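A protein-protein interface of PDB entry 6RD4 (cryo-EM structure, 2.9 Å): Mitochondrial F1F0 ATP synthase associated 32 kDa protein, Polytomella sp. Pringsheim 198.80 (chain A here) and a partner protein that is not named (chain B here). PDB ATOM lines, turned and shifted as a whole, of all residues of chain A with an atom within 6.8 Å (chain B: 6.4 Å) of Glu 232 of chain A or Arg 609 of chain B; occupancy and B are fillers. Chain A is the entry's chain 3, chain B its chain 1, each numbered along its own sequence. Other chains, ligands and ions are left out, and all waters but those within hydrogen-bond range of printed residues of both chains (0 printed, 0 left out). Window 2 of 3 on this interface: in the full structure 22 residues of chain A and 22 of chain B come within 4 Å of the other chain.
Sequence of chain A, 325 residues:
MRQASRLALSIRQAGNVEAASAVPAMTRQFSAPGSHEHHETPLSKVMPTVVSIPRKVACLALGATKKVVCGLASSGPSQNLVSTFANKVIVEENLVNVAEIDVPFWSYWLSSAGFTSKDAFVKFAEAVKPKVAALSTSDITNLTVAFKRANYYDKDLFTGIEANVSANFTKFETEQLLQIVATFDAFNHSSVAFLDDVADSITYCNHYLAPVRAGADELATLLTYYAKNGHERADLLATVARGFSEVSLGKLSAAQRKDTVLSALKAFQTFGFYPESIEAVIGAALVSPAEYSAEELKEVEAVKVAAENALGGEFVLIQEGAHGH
Printed residues of chain B within 4 Å of Asp 196 of chain A: Arg 600 and Arg 604. Printed residues of chain B within 4 Å of Arg 233 of chain A: Arg 600 (3.4 Å) and Asp 613 (3.4 Å). Of the printed residues of chain B, Asp 235 of chain A touches Asp 613. Gly 272 of chain A touches none of the printed residues of chain B. Of chain A, only Glu 232 comes within 4 Å of Arg 609 of chain B. Of the printed residues of chain A, Leu 614 of chain B touches Glu 232 (3.3 Å) and Ala 234 (3.6 Å). Printed residues of chain A within 4 Å of Val 615 of chain B: Glu 232, Ala 234 and Phe 271. The nearest residue of chain A that does not touch Arg 609 of chain B is Gly 230 of chain A (5.5 Å).
Arg 600 of chain B touches Asp 196 of chain A (CD to OD2, 3.9 Å). Glu 232 of chain A touches Leu 614 of chain B. CB of Ala 234 of chain A touches C of Leu 614 of chain B, 3.6 Å away. Val 615 of chain B touches Ala 234 of chain A. Asp 235 of chain A touches Asp 613 of chain B. Phe 271 of chain A touches Val 615 of chain B.
The guanidinium group of Arg 600 of chain B is in salt-bridge range of the side-chain carboxylate of Asp 613 of chain B, 3.0 Å away. OD1 of Asp 196 of chain A lies within salt-bridge range of NH2 of Arg 233 of chain A (3.1 Å). OD2 of Asp 235 of chain A is in salt-bridge range of NH1 of Arg 233 of chain A.
The guanidinium group of Arg 604 of chain B is in salt-bridge range of the side-chain carboxylate of Asp 196 of chain A (3.5 Å). The side-chain carboxylate (OE1) of Glu 232 of chain A is in salt-bridge range of the guanidinium group (NH1) of Arg 609 of chain B (3.7 Å). The side-chain carboxylate (OD1) of Asp 613 of chain B lies within salt-bridge range of the guanidinium group (NE) of Arg 233 of chain A (3.8 Å). The backbone carbonyl oxygen (O) of Asp 613 of chain B sits at hydrogen-bond distance from the backbone NH (N) of Ala 234 of chain A (2.5 Å). The side-chain carboxylate (OE2) of Glu 232 of chain A sits at hydrogen-bond distance from the backbone NH (N) of Val 615 of chain B, at 2.6 Å. The backbone carbonyl oxygen of Asp 613 of chain B sits close to the backbone carbonyl oxygen of Glu 232 of chain A (3.2 Å). The guanidinium group (NH1) of Arg 233 of chain A lies close to the guanidinium group (NH2) of Arg 600 of chain B (3.4 Å).
Of the 13 printed residues of chain B, 6 touch a printed residue of chain A. Printed residues of chain B that touch a printed residue of chain A: Arg 600, Arg 604, Arg 609, Asp 613, Leu 614 and Val 615. Hydrophobic or aromatic side chains of chain B that line the printed part of chain A: Leu 614 and Val 615. Along chain B the printed residues that touch a printed residue of chain A span positions 600 to 615. Of the 13 printed residues of chain A, 6 touch a printed residue of chain B. Among the printed residues, Asp or Glu carboxylates within 4 Å of a Lys or Arg side-chain nitrogen of the other chain: Asp 196 of chain A with Arg 604 of chain B (3.5 Å), Glu 232 of chain A with Arg 609 of chain B (3.7 Å) and Arg 233 of chain A with Asp 613 of chain B (3.8 Å).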
ATOM      1  N   ASP A 196      -0.163 -17.139  17.596  1.00  0.00           N
ATOM      2  CA  ASP A 196       1.016 -17.964  17.421  1.00  0.00           C
ATOM      3  C   ASP A 196       1.063 -19.092  18.432  1.00  0.00           C
ATOM      4  O   ASP A 196       1.406 -20.214  18.074  1.00  0.00           O
ATOM      5  CB  ASP A 196       2.269 -17.110  17.533  1.00  0.00           C
ATOM      6  CG  ASP A 196       2.667 -16.496  16.219  1.00  0.00           C
ATOM      7  OD1 ASP A 196       2.441 -17.124  15.174  1.00  0.00           O
ATOM      8  OD2 ASP A 196       3.225 -15.389  16.226  1.00  0.00           O
ATOM      9  N   TYR A 226      -8.031 -17.846  11.602  1.00  0.00           N
ATOM     10  CA  TYR A 226      -6.714 -17.462  11.140  1.00  0.00           C
ATOM     11  C   TYR A 226      -6.764 -16.701   9.834  1.00  0.00           C
ATOM     12  O   TYR A 226      -5.784 -16.045   9.483  1.00  0.00           O
ATOM     13  CB  TYR A 226      -5.812 -18.693  11.003  1.00  0.00           C
ATOM     14  CG  TYR A 226      -5.149 -19.029  12.311  1.00  0.00           C
ATOM     15  CD1 TYR A 226      -3.807 -18.788  12.517  1.00  0.00           C
ATOM     16  CD2 TYR A 226      -5.886 -19.538  13.359  1.00  0.00           C
ATOM     17  CE1 TYR A 226      -3.231 -19.059  13.715  1.00  0.00           C
ATOM     18  CE2 TYR A 226      -5.313 -19.811  14.553  1.00  0.00           C
ATOM     19  CZ  TYR A 226      -3.992 -19.572  14.725  1.00  0.00           C
ATOM     20  OH  TYR A 226      -3.424 -19.850  15.928  1.00  0.00           O
ATOM     21  N   ASN A 229      -8.146 -12.938  10.924  1.00  0.00           N
ATOM     22  CA  ASN A 229      -7.073 -12.163  11.514  1.00  0.00           C
ATOM     23  C   ASN A 229      -5.839 -12.094  10.632  1.00  0.00           C
ATOM     24  O   ASN A 229      -4.825 -11.546  11.061  1.00  0.00           O
ATOM     25  CB  ASN A 229      -6.724 -12.734  12.880  1.00  0.00           C
ATOM     26  CG  ASN A 229      -7.829 -12.533  13.877  1.00  0.00           C
ATOM     27  OD1 ASN A 229      -8.588 -13.441  14.169  1.00  0.00           O
ATOM     28  ND2 ASN A 229      -7.914 -11.341  14.419  1.00  0.00           N
ATOM     29  N   GLY A 230      -5.903 -12.646   9.424  1.00  0.00           N
ATOM     30  CA  GLY A 230      -4.838 -12.480   8.454  1.00  0.00           C
ATOM     31  C   GLY A 230      -3.541 -13.151   8.821  1.00  0.00           C
ATOM     32  O   GLY A 230      -2.474 -12.697   8.403  1.00  0.00           O
ATOM     33  N   HIS A 231      -3.605 -14.223   9.599  1.00  0.00           N
ATOM     34  CA  HIS A 231      -2.436 -14.858  10.187  1.00  0.00           C
ATOM     35  C   HIS A 231      -2.083 -16.073   9.356  1.00  0.00           C
ATOM     36  O   HIS A 231      -2.817 -17.058   9.352  1.00  0.00           O
ATOM     37  CB  HIS A 231      -2.729 -15.248  11.627  1.00  0.00           C
ATOM     38  CG  HIS A 231      -1.539 -15.177  12.517  1.00  0.00           C
ATOM     39  ND1 HIS A 231      -0.483 -16.049  12.411  1.00  0.00           N
ATOM     40  CD2 HIS A 231      -1.233 -14.339  13.532  1.00  0.00           C
ATOM     41  CE1 HIS A 231       0.423 -15.751  13.320  1.00  0.00           C
ATOM     42  NE2 HIS A 231      -0.009 -14.719  14.016  1.00  0.00           N
ATOM     43  N   GLU A 232      -0.972 -16.008   8.644  1.00  0.00           N
ATOM     44  CA  GLU A 232      -0.550 -17.110   7.795  1.00  0.00           C
ATOM     45  C   GLU A 232       0.482 -17.928   8.548  1.00  0.00           C
ATOM     46  O   GLU A 232       1.622 -17.490   8.728  1.00  0.00           O
ATOM     47  CB  GLU A 232       0.014 -16.600   6.479  1.00  0.00           C
ATOM     48  CG  GLU A 232       0.433 -17.697   5.536  1.00  0.00           C
ATOM     49  CD  GLU A 232       0.976 -17.156   4.231  1.00  0.00           C
ATOM     50  OE1 GLU A 232       0.643 -16.009   3.869  1.00  0.00           O
ATOM     51  OE2 GLU A 232       1.746 -17.872   3.570  1.00  0.00           O
ATOM     52  N   ARG A 233       0.074 -19.113   9.000  1.00  0.00           N
ATOM     53  CA  ARG A 233       0.941 -20.092   9.645  1.00  0.00           C
ATOM     54  C   ARG A 233       0.835 -21.315   8.762  1.00  0.00           C
ATOM     55  O   ARG A 233      -0.106 -22.080   8.919  1.00  0.00           O
ATOM     56  CB  ARG A 233       0.485 -20.392  11.052  1.00  0.00           C
ATOM     57  CG  ARG A 233       0.666 -19.286  12.038  1.00  0.00           C
ATOM     58  CD  ARG A 233       2.101 -19.159  12.410  1.00  0.00           C
ATOM     59  NE  ARG A 233       2.680 -20.461  12.659  1.00  0.00           N
ATOM     60  CZ  ARG A 233       2.895 -20.952  13.864  1.00  0.00           C
ATOM     61  NH1 ARG A 233       3.427 -22.147  14.003  1.00  0.00           N
ATOM     62  NH2 ARG A 233       2.588 -20.236  14.922  1.00  0.00           N
ATOM     63  N   ALA A 234       1.771 -21.506   7.840  1.00  0.00           N
ATOM     64  CA  ALA A 234       1.637 -22.604   6.892  1.00  0.00           C
ATOM     65  C   ALA A 234       1.890 -23.954   7.524  1.00  0.00           C
ATOM     66  O   ALA A 234       1.581 -24.976   6.909  1.00  0.00           O
ATOM     67  CB  ALA A 234       2.589 -22.426   5.723  1.00  0.00           C
ATOM     68  N   ASP A 235       2.483 -23.984   8.711  1.00  0.00           N
ATOM     69  CA  ASP A 235       2.645 -25.235   9.431  1.00  0.00           C
ATOM     70  C   ASP A 235       1.351 -25.656  10.106  1.00  0.00           C
ATOM     71  O   ASP A 235       1.044 -26.848  10.166  1.00  0.00           O
ATOM     72  CB  ASP A 235       3.791 -25.101  10.426  1.00  0.00           C
ATOM     73  CG  ASP A 235       3.676 -23.878  11.296  1.00  0.00           C
ATOM     74  OD1 ASP A 235       2.712 -23.125  11.168  1.00  0.00           O
ATOM     75  OD2 ASP A 235       4.583 -23.632  12.101  1.00  0.00           O
ATOM     76  N   LEU A 237      -1.617 -24.903   8.934  1.00  0.00           N
ATOM     77  CA  LEU A 237      -2.582 -25.264   7.913  1.00  0.00           C
ATOM     78  C   LEU A 237      -2.357 -26.668   7.392  1.00  0.00           C
ATOM     79  O   LEU A 237      -3.300 -27.296   6.924  1.00  0.00           O
ATOM     80  CB  LEU A 237      -2.522 -24.286   6.755  1.00  0.00           C
ATOM     81  CG  LEU A 237      -2.669 -22.813   7.069  1.00  0.00           C
ATOM     82  CD1 LEU A 237      -2.459 -22.028   5.813  1.00  0.00           C
ATOM     83  CD2 LEU A 237      -4.006 -22.534   7.681  1.00  0.00           C
ATOM     84  N   THR A 270      -7.646 -18.014   1.035  1.00  0.00           N
ATOM     85  CA  THR A 270      -7.156 -16.778   1.631  1.00  0.00           C
ATOM     86  C   THR A 270      -5.659 -16.841   1.884  1.00  0.00           C
ATOM     87  O   THR A 270      -4.968 -15.823   1.800  1.00  0.00           O
ATOM     88  CB  THR A 270      -7.918 -16.502   2.921  1.00  0.00           C
ATOM     89  OG1 THR A 270      -9.317 -16.620   2.660  1.00  0.00           O
ATOM     90  CG2 THR A 270      -7.652 -15.121   3.440  1.00  0.00           C
ATOM     91  N   PHE A 271      -5.133 -18.024   2.162  1.00  0.00           N
ATOM     92  CA  PHE A 271      -3.700 -18.216   2.255  1.00  0.00           C
ATOM     93  C   PHE A 271      -3.102 -18.789   0.991  1.00  0.00           C
ATOM     94  O   PHE A 271      -1.882 -18.760   0.839  1.00  0.00           O
ATOM     95  CB  PHE A 271      -3.373 -19.132   3.422  1.00  0.00           C
ATOM     96  CG  PHE A 271      -4.008 -18.712   4.684  1.00  0.00           C
ATOM     97  CD1 PHE A 271      -3.621 -17.546   5.304  1.00  0.00           C
ATOM     98  CD2 PHE A 271      -5.006 -19.465   5.240  1.00  0.00           C
ATOM     99  CE1 PHE A 271      -4.212 -17.151   6.456  1.00  0.00           C
ATOM    100  CE2 PHE A 271      -5.607 -19.075   6.386  1.00  0.00           C
ATOM    101  CZ  PHE A 271      -5.203 -17.922   7.000  1.00  0.00           C
ATOM    102  N   GLY A 272      -3.923 -19.293   0.079  1.00  0.00           N
ATOM    103  CA  GLY A 272      -3.372 -19.886  -1.112  1.00  0.00           C
ATOM    104  C   GLY A 272      -2.712 -21.205  -0.851  1.00  0.00           C
ATOM    105  O   GLY A 272      -1.813 -21.604  -1.590  1.00  0.00           O
ATOM    106  N   ARG B 600      11.420 -16.800  15.056  1.00  0.00           N
ATOM    107  CA  ARG B 600      10.251 -16.012  14.714  1.00  0.00           C
ATOM    108  C   ARG B 600      10.191 -14.727  15.516  1.00  0.00           C
ATOM    109  O   ARG B 600       9.707 -13.716  15.013  1.00  0.00           O
ATOM    110  CB  ARG B 600       8.993 -16.839  14.936  1.00  0.00           C
ATOM    111  CG  ARG B 600       7.715 -16.213  14.483  1.00  0.00           C
ATOM    112  CD  ARG B 600       6.545 -16.960  15.037  1.00  0.00           C
ATOM    113  NE  ARG B 600       6.559 -18.352  14.632  1.00  0.00           N
ATOM    114  CZ  ARG B 600       6.207 -19.360  15.418  1.00  0.00           C
ATOM    115  NH1 ARG B 600       5.816 -19.135  16.658  1.00  0.00           N
ATOM    116  NH2 ARG B 600       6.250 -20.596  14.960  1.00  0.00           N
ATOM    117  N   ALA B 603      12.700 -12.301  13.826  1.00  0.00           N
ATOM    118  CA  ALA B 603      12.186 -11.697  12.611  1.00  0.00           C
ATOM    119  C   ALA B 603      10.968 -10.829  12.854  1.00  0.00           C
ATOM    120  O   ALA B 603      10.687  -9.955  12.038  1.00  0.00           O
ATOM    121  CB  ALA B 603      11.853 -12.779  11.597  1.00  0.00           C
ATOM    122  N   ARG B 604      10.246 -11.031  13.947  1.00  0.00           N
ATOM    123  CA  ARG B 604       9.150 -10.122  14.240  1.00  0.00           C
ATOM    124  C   ARG B 604       9.660  -8.804  14.786  1.00  0.00           C
ATOM    125  O   ARG B 604       9.130  -7.745  14.444  1.00  0.00           O
ATOM    126  CB  ARG B 604       8.177 -10.748  15.226  1.00  0.00           C
ATOM    127  CG  ARG B 604       6.890  -9.985  15.376  1.00  0.00           C
ATOM    128  CD  ARG B 604       5.843 -10.846  16.014  1.00  0.00           C
ATOM    129  NE  ARG B 604       5.742 -12.141  15.356  1.00  0.00           N
ATOM    130  CZ  ARG B 604       4.948 -12.394  14.326  1.00  0.00           C
ATOM    131  NH1 ARG B 604       4.175 -11.441  13.835  1.00  0.00           N
ATOM    132  NH2 ARG B 604       4.918 -13.601  13.786  1.00  0.00           N
ATOM    133  N   GLY B 607      11.076  -6.651  12.065  1.00  0.00           N
ATOM    134  CA  GLY B 607      10.121  -6.222  11.075  1.00  0.00           C
ATOM    135  C   GLY B 607       9.758  -7.237  10.017  1.00  0.00           C
ATOM    136  O   GLY B 607       8.737  -7.065   9.350  1.00  0.00           O
ATOM    137  N   ASP B 608      10.542  -8.289   9.841  1.00  0.00           N
ATOM    138  CA  ASP B 608      10.322  -9.222   8.751  1.00  0.00           C
ATOM    139  C   ASP B 608       9.260 -10.245   9.138  1.00  0.00           C
ATOM    140  O   ASP B 608       8.575 -10.124  10.154  1.00  0.00           O
ATOM    141  CB  ASP B 608      11.629  -9.906   8.369  1.00  0.00           C
ATOM    142  CG  ASP B 608      12.729  -8.923   8.066  1.00  0.00           C
ATOM    143  OD1 ASP B 608      12.433  -7.865   7.479  1.00  0.00           O
ATOM    144  OD2 ASP B 608      13.888  -9.200   8.424  1.00  0.00           O
ATOM    145  N   ARG B 609       9.096 -11.254   8.303  1.00  0.00           N
ATOM    146  CA  ARG B 609       8.250 -12.387   8.612  1.00  0.00           C
ATOM    147  C   ARG B 609       9.137 -13.609   8.744  1.00  0.00           C
ATOM    148  O   ARG B 609      10.208 -13.678   8.139  1.00  0.00           O
ATOM    149  CB  ARG B 609       7.205 -12.625   7.531  1.00  0.00           C
ATOM    150  CG  ARG B 609       6.261 -11.475   7.325  1.00  0.00           C
ATOM    151  CD  ARG B 609       5.545 -11.636   6.015  1.00  0.00           C
ATOM    152  NE  ARG B 609       4.166 -12.065   6.179  1.00  0.00           N
ATOM    153  CZ  ARG B 609       3.448 -12.628   5.216  1.00  0.00           C
ATOM    154  NH1 ARG B 609       2.196 -12.985   5.442  1.00  0.00           N
ATOM    155  NH2 ARG B 609       3.988 -12.848   4.028  1.00  0.00           N
ATOM    156  N   TYR B 610       8.700 -14.567   9.550  1.00  0.00           N
ATOM    157  CA  TYR B 610       9.436 -15.814   9.622  1.00  0.00           C
ATOM    158  C   TYR B 610       9.215 -16.588   8.337  1.00  0.00           C
ATOM    159  O   TYR B 610       8.091 -16.681   7.844  1.00  0.00           O
ATOM    160  CB  TYR B 610       9.010 -16.635  10.828  1.00  0.00           C
ATOM    161  CG  TYR B 610       9.961 -17.757  11.113  1.00  0.00           C
ATOM    162  CD1 TYR B 610      11.314 -17.600  10.899  1.00  0.00           C
ATOM    163  CD2 TYR B 610       9.510 -18.974  11.578  1.00  0.00           C
ATOM    164  CE1 TYR B 610      12.186 -18.615  11.141  1.00  0.00           C
ATOM    165  CE2 TYR B 610      10.381 -20.000  11.819  1.00  0.00           C
ATOM    166  CZ  TYR B 610      11.716 -19.811  11.604  1.00  0.00           C
ATOM    167  OH  TYR B 610      12.596 -20.834  11.846  1.00  0.00           O
ATOM    168  N   GLY B 611      10.299 -17.113   7.789  1.00  0.00           N
ATOM    169  CA  GLY B 611      10.302 -17.825   6.536  1.00  0.00           C
ATOM    170  C   GLY B 611       9.389 -19.027   6.454  1.00  0.00           C
ATOM    171  O   GLY B 611       8.480 -19.064   5.626  1.00  0.00           O
ATOM    172  N   ASP B 613       6.964 -19.984   8.256  1.00  0.00           N
ATOM    173  CA  ASP B 613       5.561 -19.794   8.588  1.00  0.00           C
ATOM    174  C   ASP B 613       4.710 -19.552   7.358  1.00  0.00           C
ATOM    175  O   ASP B 613       3.495 -19.735   7.421  1.00  0.00           O
ATOM    176  CB  ASP B 613       5.381 -18.611   9.533  1.00  0.00           C
ATOM    177  CG  ASP B 613       5.747 -18.934  10.954  1.00  0.00           C
ATOM    178  OD1 ASP B 613       6.137 -20.080  11.226  1.00  0.00           O
ATOM    179  OD2 ASP B 613       5.643 -18.034  11.807  1.00  0.00           O
ATOM    180  N   LEU B 614       5.311 -19.138   6.253  1.00  0.00           N
ATOM    181  CA  LEU B 614       4.596 -18.707   5.065  1.00  0.00           C
ATOM    182  C   LEU B 614       4.484 -19.849   4.073  1.00  0.00           C
ATOM    183  O   LEU B 614       5.308 -20.761   4.050  1.00  0.00           O
ATOM    184  CB  LEU B 614       5.311 -17.534   4.402  1.00  0.00           C
ATOM    185  CG  LEU B 614       5.883 -16.500   5.355  1.00  0.00           C
ATOM    186  CD1 LEU B 614       6.719 -15.525   4.588  1.00  0.00           C
ATOM    187  CD2 LEU B 614       4.774 -15.791   6.094  1.00  0.00           C
ATOM    188  N   VAL B 615       3.451 -19.778   3.236  1.00  0.00           N
ATOM    189  CA  VAL B 615       3.207 -20.842   2.270  1.00  0.00           C
ATOM    190  C   VAL B 615       4.253 -20.806   1.166  1.00  0.00           C
ATOM    191  O   VAL B 615       4.992 -21.771   0.951  1.00  0.00           O
ATOM    192  CB  VAL B 615       1.790 -20.728   1.697  1.00  0.00           C
ATOM    193  CG1 VAL B 615       1.590 -21.772   0.648  1.00  0.00           C
ATOM    194  CG2 VAL B 615       0.779 -20.892   2.788  1.00  0.00           C
ATOM    195  N   ASN B 616       4.335 -19.687   0.456  1.00  0.00           N
ATOM    196  CA  ASN B 616       5.280 -19.563  -0.641  1.00  0.00           C
ATOM    197  C   ASN B 616       6.684 -19.245  -0.160  1.00  0.00           C
ATOM    198  O   ASN B 616       7.644 -19.491  -0.894  1.00  0.00           O
ATOM    199  CB  ASN B 616       4.810 -18.484  -1.610  1.00  0.00           C
ATOM    200  CG  ASN B 616       3.313 -18.508  -1.821  1.00  0.00           C
ATOM    201  OD1 ASN B 616       2.574 -17.768  -1.174  1.00  0.00           O
ATOM    202  ND2 ASN B 616       2.857 -19.369  -2.719  1.00  0.00           N
ATOM    203  N   GLY B 617       6.824 -18.710   1.046  1.00  0.00           N
ATOM    204  CA  GLY B 617       8.128 -18.426   1.613  1.00  0.00           C
ATOM    205  C   GLY B 617       8.711 -19.625   2.331  1.00  0.00           C
ATOM    206  O   GLY B 617       8.747 -20.724   1.783  1.00  0.00           O
